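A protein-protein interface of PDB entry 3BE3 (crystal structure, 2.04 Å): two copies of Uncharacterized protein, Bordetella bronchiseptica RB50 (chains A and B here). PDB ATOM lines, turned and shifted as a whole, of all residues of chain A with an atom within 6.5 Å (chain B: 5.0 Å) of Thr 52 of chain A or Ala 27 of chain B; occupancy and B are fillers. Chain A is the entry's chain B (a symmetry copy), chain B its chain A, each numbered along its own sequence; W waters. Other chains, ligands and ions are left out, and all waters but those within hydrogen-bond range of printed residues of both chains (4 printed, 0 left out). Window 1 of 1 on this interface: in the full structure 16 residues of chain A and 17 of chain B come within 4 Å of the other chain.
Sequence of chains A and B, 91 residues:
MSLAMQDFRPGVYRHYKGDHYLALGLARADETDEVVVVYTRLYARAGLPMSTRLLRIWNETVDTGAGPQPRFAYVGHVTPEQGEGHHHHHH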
ATOM      1  N   VAL A  36       9.394 -16.945  22.297  1.00  0.00           N
ATOM      2  CA  VAL A  36       8.737 -16.848  23.601  1.00  0.00           C
ATOM      3  C   VAL A  36       7.542 -17.796  23.766  1.00  0.00           C
ATOM      4  O   VAL A  36       6.955 -18.251  22.783  1.00  0.00           O
ATOM      5  CB  VAL A  36       8.224 -15.404  23.845  1.00  0.00           C
ATOM      6  CG1 VAL A  36       9.361 -14.406  23.723  1.00  0.00           C
ATOM      7  CG2 VAL A  36       7.124 -15.071  22.833  1.00  0.00           C
ATOM      8  N   VAL A  37       7.184 -18.081  25.017  1.00  0.00           N
ATOM      9  CA  VAL A  37       6.028 -18.928  25.316  1.00  0.00           C
ATOM     10  C   VAL A  37       4.871 -17.982  25.644  1.00  0.00           C
ATOM     11  O   VAL A  37       5.039 -17.027  26.406  1.00  0.00           O
ATOM     12  CB  VAL A  37       6.272 -19.853  26.555  1.00  0.00           C
ATOM     13  CG1 VAL A  37       4.990 -20.624  26.917  1.00  0.00           C
ATOM     14  CG2 VAL A  37       7.417 -20.821  26.270  1.00  0.00           C
ATOM     15  N   VAL A  38       3.711 -18.238  25.043  1.00  0.00           N
ATOM     16  CA  VAL A  38       2.502 -17.448  25.277  1.00  0.00           C
ATOM     17  C   VAL A  38       1.668 -18.298  26.229  1.00  0.00           C
ATOM     18  O   VAL A  38       1.332 -19.437  25.903  1.00  0.00           O
ATOM     19  CB  VAL A  38       1.708 -17.223  23.965  1.00  0.00           C
ATOM     20  CG1 VAL A  38       0.409 -16.471  24.256  1.00  0.00           C
ATOM     21  CG2 VAL A  38       2.562 -16.435  22.984  1.00  0.00           C
ATOM     22  N   TYR A  39       1.345 -17.760  27.402  1.00  0.00           N
ATOM     23  CA  TYR A  39       0.582 -18.522  28.388  1.00  0.00           C
ATOM     24  C   TYR A  39      -0.404 -17.692  29.217  1.00  0.00           C
ATOM     25  O   TYR A  39      -0.242 -16.480  29.373  1.00  0.00           O
ATOM     26  CB  TYR A  39       1.557 -19.261  29.316  1.00  0.00           C
ATOM     27  CG  TYR A  39       2.486 -18.385  30.149  1.00  0.00           C
ATOM     28  CD1 TYR A  39       2.297 -18.237  31.522  1.00  0.00           C
ATOM     29  CD2 TYR A  39       3.578 -17.740  29.577  1.00  0.00           C
ATOM     30  CE1 TYR A  39       3.174 -17.471  32.304  1.00  0.00           C
ATOM     31  CE2 TYR A  39       4.459 -16.973  30.354  1.00  0.00           C
ATOM     32  CZ  TYR A  39       4.256 -16.843  31.714  1.00  0.00           C
ATOM     33  OH  TYR A  39       5.151 -16.114  32.475  1.00  0.00           O
ATOM     34  N   LEU A  48      -3.285  -8.431  33.777  1.00  0.00           N
ATOM     35  CA  LEU A  48      -3.385  -9.062  32.470  1.00  0.00           C
ATOM     36  C   LEU A  48      -3.284 -10.571  32.684  1.00  0.00           C
ATOM     37  O   LEU A  48      -2.329 -11.048  33.289  1.00  0.00           O
ATOM     38  CB  LEU A  48      -2.241  -8.577  31.571  1.00  0.00           C
ATOM     39  CG  LEU A  48      -2.371  -7.140  31.050  1.00  0.00           C
ATOM     40  CD1 LEU A  48      -1.039  -6.662  30.508  1.00  0.00           C
ATOM     41  CD2 LEU A  48      -3.442  -7.079  29.979  1.00  0.00           C
ATOM     42  N   PRO A  49      -4.282 -11.338  32.216  1.00  0.00           N
ATOM     43  CA  PRO A  49      -4.197 -12.788  32.412  1.00  0.00           C
ATOM     44  C   PRO A  49      -3.144 -13.481  31.545  1.00  0.00           C
ATOM     45  O   PRO A  49      -2.577 -14.495  31.956  1.00  0.00           O
ATOM     46  CB  PRO A  49      -5.627 -13.268  32.126  1.00  0.00           C
ATOM     47  CG  PRO A  49      -6.172 -12.239  31.194  1.00  0.00           C
ATOM     48  CD  PRO A  49      -5.632 -10.943  31.777  1.00  0.00           C
ATOM     49  N   MET A  50      -2.870 -12.940  30.358  1.00  0.00           N
ATOM     50  CA  MET A  50      -1.867 -13.545  29.483  1.00  0.00           C
ATOM     51  C   MET A  50      -0.485 -12.956  29.705  1.00  0.00           C
ATOM     52  O   MET A  50      -0.340 -11.774  30.046  1.00  0.00           O
ATOM     53  CB  MET A  50      -2.242 -13.400  28.000  1.00  0.00           C
ATOM     54  CG  MET A  50      -3.281 -14.390  27.521  1.00  0.00           C
ATOM     55  SD  MET A  50      -3.195 -14.688  25.599  1.00  0.00           S
ATOM     56  CE  MET A  50      -3.991 -13.013  25.039  1.00  0.00           C
ATOM     57  N   SER A  51       0.529 -13.791  29.496  1.00  0.00           N
ATOM     58  CA  SER A  51       1.914 -13.375  29.667  1.00  0.00           C
ATOM     59  C   SER A  51       2.776 -14.027  28.599  1.00  0.00           C
ATOM     60  O   SER A  51       2.342 -14.969  27.940  1.00  0.00           O
ATOM     61  CB  SER A  51       2.427 -13.814  31.047  1.00  0.00           C
ATOM     62  OG  SER A  51       1.634 -13.292  32.097  1.00  0.00           O
ATOM     63  N   THR A  52       3.995 -13.519  28.417  1.00  0.00           N
ATOM     64  CA  THR A  52       4.923 -14.115  27.461  1.00  0.00           C
ATOM     65  C   THR A  52       6.266 -14.218  28.177  1.00  0.00           C
ATOM     66  O   THR A  52       6.624 -13.354  28.983  1.00  0.00           O
ATOM     67  CB  THR A  52       5.111 -13.271  26.172  1.00  0.00           C
ATOM     68  OG1 THR A  52       5.872 -12.094  26.475  1.00  0.00           O
ATOM     69  CG2 THR A  52       3.766 -12.884  25.578  1.00  0.00           C
ATOM     70  N   ARG A  53       7.004 -15.286  27.900  1.00  0.00           N
ATOM     71  CA  ARG A  53       8.302 -15.488  28.537  1.00  0.00           C
ATOM     72  C   ARG A  53       9.223 -16.250  27.599  1.00  0.00           C
ATOM     73  O   ARG A  53       8.796 -17.195  26.937  1.00  0.00           O
ATOM     74  CB  ARG A  53       8.133 -16.264  29.841  1.00  0.00           C
ATOM     75  CG  ARG A  53       9.371 -16.267  30.712  1.00  0.00           C
ATOM     76  CD  ARG A  53       9.040 -16.689  32.136  1.00  0.00           C
ATOM     77  NE  ARG A  53      10.151 -16.436  33.047  1.00  0.00           N
ATOM     78  CZ  ARG A  53      10.084 -16.592  34.365  1.00  0.00           C
ATOM     79  NH1 ARG A  53       8.955 -17.004  34.926  1.00  0.00           N
ATOM     80  NH2 ARG A  53      11.146 -16.335  35.113  1.00  0.00           N
ATOM     81  N   LEU A  54      10.488 -15.839  27.550  1.00  0.00           N
ATOM     82  CA  LEU A  54      11.466 -16.493  26.690  1.00  0.00           C
ATOM     83  C   LEU A  54      11.433 -18.004  26.901  1.00  0.00           C
ATOM     84  O   LEU A  54      11.380 -18.489  28.031  1.00  0.00           O
ATOM     85  CB  LEU A  54      12.877 -15.954  26.982  1.00  0.00           C
ATOM     86  CG  LEU A  54      13.114 -14.474  26.665  1.00  0.00           C
ATOM     87  CD1 LEU A  54      14.444 -14.021  27.245  1.00  0.00           C
ATOM     88  CD2 LEU A  54      13.077 -14.264  25.151  1.00  0.00           C
ATOM     89  N   GLY B  25      -5.299 -10.992  21.844  1.00  0.00           N
ATOM     90  CA  GLY B  25      -5.451 -10.187  23.043  1.00  0.00           C
ATOM     91  C   GLY B  25      -4.142  -9.571  23.485  1.00  0.00           C
ATOM     92  O   GLY B  25      -3.146  -9.630  22.761  1.00  0.00           O
ATOM     93  N   LEU B  26      -4.143  -8.971  24.671  1.00  0.00           N
ATOM     94  CA  LEU B  26      -2.952  -8.344  25.219  1.00  0.00           C
ATOM     95  C   LEU B  26      -2.293  -9.304  26.203  1.00  0.00           C
ATOM     96  O   LEU B  26      -2.939 -10.211  26.731  1.00  0.00           O
ATOM     97  CB  LEU B  26      -3.323  -7.043  25.938  1.00  0.00           C
ATOM     98  CG  LEU B  26      -3.918  -5.942  25.059  1.00  0.00           C
ATOM     99  CD1 LEU B  26      -4.255  -4.713  25.903  1.00  0.00           C
ATOM    100  CD2 LEU B  26      -2.923  -5.580  23.964  1.00  0.00           C
ATOM    101  N   ALA B  27      -0.998  -9.102  26.430  1.00  0.00           N
ATOM    102  CA  ALA B  27      -0.238  -9.934  27.362  1.00  0.00           C
ATOM    103  C   ALA B  27       0.875  -9.121  28.004  1.00  0.00           C
ATOM    104  O   ALA B  27       1.253  -8.059  27.507  1.00  0.00           O
ATOM    105  CB  ALA B  27       0.359 -11.146  26.631  1.00  0.00           C
ATOM    106  N   ARG B  28       1.387  -9.628  29.120  1.00  0.00           N
ATOM    107  CA  ARG B  28       2.473  -8.984  29.840  1.00  0.00           C
ATOM    108  C   ARG B  28       3.773  -9.721  29.518  1.00  0.00           C
ATOM    109  O   ARG B  28       3.891 -10.922  29.759  1.00  0.00           O
ATOM    110  CB  ARG B  28       2.202  -9.030  31.348  1.00  0.00           C
ATOM    111  CG  ARG B  28       3.375  -8.605  32.234  1.00  0.00           C
ATOM    112  CD  ARG B  28       3.069  -8.810  33.727  1.00  0.00           C
ATOM    113  NE  ARG B  28       4.262  -9.229  34.466  1.00  0.00           N
ATOM    114  CZ  ARG B  28       4.730 -10.476  34.473  1.00  0.00           C
ATOM    115  NH1 ARG B  28       4.104 -11.427  33.792  1.00  0.00           N
ATOM    116  NH2 ARG B  28       5.834 -10.772  35.149  1.00  0.00           N
ATOM    117  N   ALA B  29       4.729  -9.008  28.935  1.00  0.00           N
ATOM    118  CA  ALA B  29       6.027  -9.596  28.618  1.00  0.00           C
ATOM    119  C   ALA B  29       6.735  -9.666  29.964  1.00  0.00           C
ATOM    120  O   ALA B  29       7.002  -8.645  30.589  1.00  0.00           O
ATOM    121  CB  ALA B  29       6.793  -8.696  27.657  1.00  0.00           C
ATOM    122  N   ASP B  30       7.033 -10.878  30.409  1.00  0.00           N
ATOM    123  CA  ASP B  30       7.655 -11.087  31.702  1.00  0.00           C
ATOM    124  C   ASP B  30       9.011 -10.423  31.945  1.00  0.00           C
ATOM    125  O   ASP B  30       9.247  -9.883  33.027  1.00  0.00           O
ATOM    126  CB  ASP B  30       7.753 -12.589  31.963  1.00  0.00           C
ATOM    127  CG  ASP B  30       7.957 -12.910  33.425  1.00  0.00           C
ATOM    128  OD1 ASP B  30       9.129 -12.969  33.862  1.00  0.00           O
ATOM    129  OD2 ASP B  30       6.943 -13.090  34.138  1.00  0.00           O
ATOM    130  N   GLU B  31       9.892 -10.454  30.948  1.00  0.00           N
ATOM    131  CA  GLU B  31      11.235  -9.877  31.095  1.00  0.00           C
ATOM    132  C   GLU B  31      11.298  -8.361  31.296  1.00  0.00           C
ATOM    133  O   GLU B  31      12.187  -7.858  31.989  1.00  0.00           O
ATOM    134  CB  GLU B  31      12.106 -10.224  29.880  1.00  0.00           C
ATOM    135  CG  GLU B  31      12.466 -11.700  29.706  1.00  0.00           C
ATOM    136  CD  GLU B  31      11.285 -12.546  29.260  1.00  0.00           C
ATOM    137  OE1 GLU B  31      10.363 -11.991  28.624  1.00  0.00           O
ATOM    138  OE2 GLU B  31      11.291 -13.767  29.529  1.00  0.00           O
ATOM    139  N   GLU B  34       6.157  -5.230  30.036  1.00  0.00           N
ATOM    140  CA  GLU B  34       5.489  -4.357  29.077  1.00  0.00           C
ATOM    141  C   GLU B  34       4.285  -5.023  28.410  1.00  0.00           C
ATOM    142  O   GLU B  34       4.207  -6.248  28.331  1.00  0.00           O
ATOM    143  CB  GLU B  34       6.505  -3.889  28.027  1.00  0.00           C
ATOM    144  CG  GLU B  34       7.695  -3.147  28.631  1.00  0.00           C
ATOM    145  CD  GLU B  34       8.765  -2.833  27.603  1.00  0.00           C
ATOM    146  OE1 GLU B  34       9.242  -3.782  26.942  1.00  0.00           O
ATOM    147  OE2 GLU B  34       9.135  -1.647  27.455  1.00  0.00           O
ATOM    148  N   VAL B  35       3.348  -4.208  27.934  1.00  0.00           N
ATOM    149  CA  VAL B  35       2.136  -4.714  27.294  1.00  0.00           C
ATOM    150  C   VAL B  35       2.378  -5.011  25.809  1.00  0.00           C
ATOM    151  O   VAL B  35       2.786  -4.132  25.046  1.00  0.00           O
ATOM    152  CB  VAL B  35       0.969  -3.693  27.447  1.00  0.00           C
ATOM    153  CG1 VAL B  35      -0.306  -4.256  26.857  1.00  0.00           C
ATOM    154  CG2 VAL B  35       0.768  -3.356  28.914  1.00  0.00           C
ATOM    155  N   VAL B  36       2.152  -6.263  25.417  1.00  0.00           N
ATOM    156  CA  VAL B  36       2.333  -6.684  24.035  1.00  0.00           C
ATOM    157  C   VAL B  36       1.025  -7.226  23.481  1.00  0.00           C
ATOM    158  O   VAL B  36       0.108  -7.549  24.234  1.00  0.00           O
ATOM    159  CB  VAL B  36       3.390  -7.812  23.909  1.00  0.00           C
ATOM    160  CG1 VAL B  36       4.747  -7.317  24.416  1.00  0.00           C
ATOM    161  CG2 VAL B  36       2.939  -9.041  24.695  1.00  0.00           C
ATOM    162  N   VAL B  38      -0.650 -10.227  21.268  1.00  0.00           N
ATOM    163  CA  VAL B  38      -0.380 -11.590  20.846  1.00  0.00           C
ATOM    164  C   VAL B  38      -1.225 -11.781  19.586  1.00  0.00           C
ATOM    165  O   VAL B  38      -2.434 -11.560  19.593  1.00  0.00           O
ATOM    166  CB  VAL B  38      -0.785 -12.600  21.967  1.00  0.00           C
ATOM    167  CG1 VAL B  38      -0.537 -14.031  21.508  1.00  0.00           C
ATOM    168  CG2 VAL B  38       0.021 -12.317  23.233  1.00  0.00           C
ATOM    169  N   THR B  52       4.363 -11.657  18.800  1.00  0.00           N
ATOM    170  CA  THR B  52       3.975 -10.707  19.833  1.00  0.00           C
ATOM    171  C   THR B  52       4.627  -9.403  19.415  1.00  0.00           C
ATOM    172  O   THR B  52       5.611  -9.390  18.668  1.00  0.00           O
ATOM    173  CB  THR B  52       4.464 -11.079  21.255  1.00  0.00           C
ATOM    174  OG1 THR B  52       5.880 -10.872  21.350  1.00  0.00           O
ATOM    175  CG2 THR B  52       4.125 -12.524  21.571  1.00  0.00           C
HETATM  176  O   HOH W   1       6.579 -11.088  23.988  1.00  0.00           O
HETATM  177  O   HOH W   2      -3.918 -10.710  29.179  1.00  0.00           O
HETATM  178  O   HOH W   3      11.810 -14.398  32.297  1.00  0.00           O
HETATM  179  O   HOH W   4       8.544 -12.392  26.779  1.00  0.00           O
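The guanidinium group (NE) of Arg 53 of chain A lies within salt-bridge range of the side-chain carboxylate (OD1) of Asp 30 of chain B (3.7 Å). N of Asp 30 of chain B lies within hydrogen-bond range of O of Thr 52 of chain A, 2.9 Å away. The backbone NH of Arg 28 of chain B lies within hydrogen-bond range of the backbone carbonyl oxygen of Met 50 of chain A (2.9 Å). The backbone carbonyl oxygen of Arg 28 of chain B sits at hydrogen-bond distance from the backbone NH of Thr 52 of chain A, at 2.9 Å. The side-chain carboxylate of Glu 31 of chain B sits at hydrogen-bond distance from the backbone NH of Leu 54 of chain A.
The backbone carbonyl oxygen (O) of Gly 25 of chain B sits at hydrogen-bond distance from the backbone NH (N) of Val 38 of chain B (3.0 Å). The backbone NH (N) of Ala 29 of chain B sits at hydrogen-bond distance from the backbone carbonyl oxygen (O) of Glu 34 of chain B (2.9 Å). The backbone NH (N) of Val 37 of chain A sits at hydrogen-bond distance from the backbone carbonyl oxygen (O) of Arg 53 of chain A, 2.7 Å away. The backbone NH (N) of Ser 51 of chain A lies within hydrogen-bond range of the backbone carbonyl oxygen (O) of Tyr 39 of chain A (2.8 Å). N of Val 36 of chain B is in hydrogen-bond range of O of Ala 27 of chain B (2.9 Å). NH2 of Arg 28 of chain B is in salt-bridge range of OD2 of Asp 30 of chain B.
OH of Tyr 39 of chain A touches OD2 of Asp 30 of chain B, at 3.9 Å. Leu 48 of chain A touches Ala 27 of chain B (CD1 to C, 3.998 Å). CE of Met 50 of chain A touches CA of Gly 25 of chain B (3.8 Å). CE of Met 50 of chain A touches O of Leu 26 of chain B, 3.4 Å away. CA of Ala 27 of chain B touches O of Met 50 of chain A, 3.3 Å away. Ala 27 of chain B touches Ser 51 of chain A (CB to N, 3.9 Å). Arg 28 of chain B touches Ser 51 of chain A. Ala 27 of chain B touches Thr 52 of chain A. Thr 52 of chain A touches Ala 29 of chain B. OE2 of Glu 31 of chain B touches CG of Arg 53 of chain A, at 3.4 Å.
Val 36 of chain A touches none of the printed residues of chain B. Printed residues of chain B within 4 Å of Val 38 of chain A: Val 38. Printed residues of chain B within 4 Å of Tyr 39 of chain A: Asp 30. Printed residues of chain B within 4 Å of Thr 52 of chain A: Ala 27, Arg 28, Ala 29, Asp 30 and Glu 31. Of the printed residues of chain A, Ala 27 of chain B touches Leu 48, Met 50, Ser 51 and Thr 52. Val 35 of chain B touches none of the printed residues of chain A. The nearest printed residue of chain A that does not touch Ala 27 of chain B is Val 38 of chain A (5.8 Å). The nearest printed residue of chain B that does not touch Met 50 of chain A is Val 38 of chain B (4.5 Å).
Along chain A the printed residues that touch a printed residue of chain B span positions 38 to 54. Among the printed residues, 17 pairs touch across the chains.
Val 38 of chain B touches its own counterpart, Val 38 of chain A. Of the 17 pairs that touch across the chains among the printed residues, 1 has its exchanged pair printed and touching as well.
Water W4 lies within hydrogen-bond range of the side-chain carboxylate (OE1) of Glu 31 of chain B, the side-chain hydroxyl (OG1) of Thr 52 of chain A and the backbone NH (N) of Arg 53 of chain A. Water W2 lies within hydrogen-bond range of the backbone carbonyl oxygen (O) of Leu 26 of chain B and the backbone NH (N) of Met 50 of chain A. Water W3 lies within hydrogen-bond range of NE of Arg 53 of chain A (2.7 Å), OE2 of Glu 31 of chain B (2.9 Å) and OD1 of Asp 30 of chain B (3.4 Å). Water W1 lies within hydrogen-bond range of OG1 of Thr 52 of chain B and OG1 of Thr 52 of chain A.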
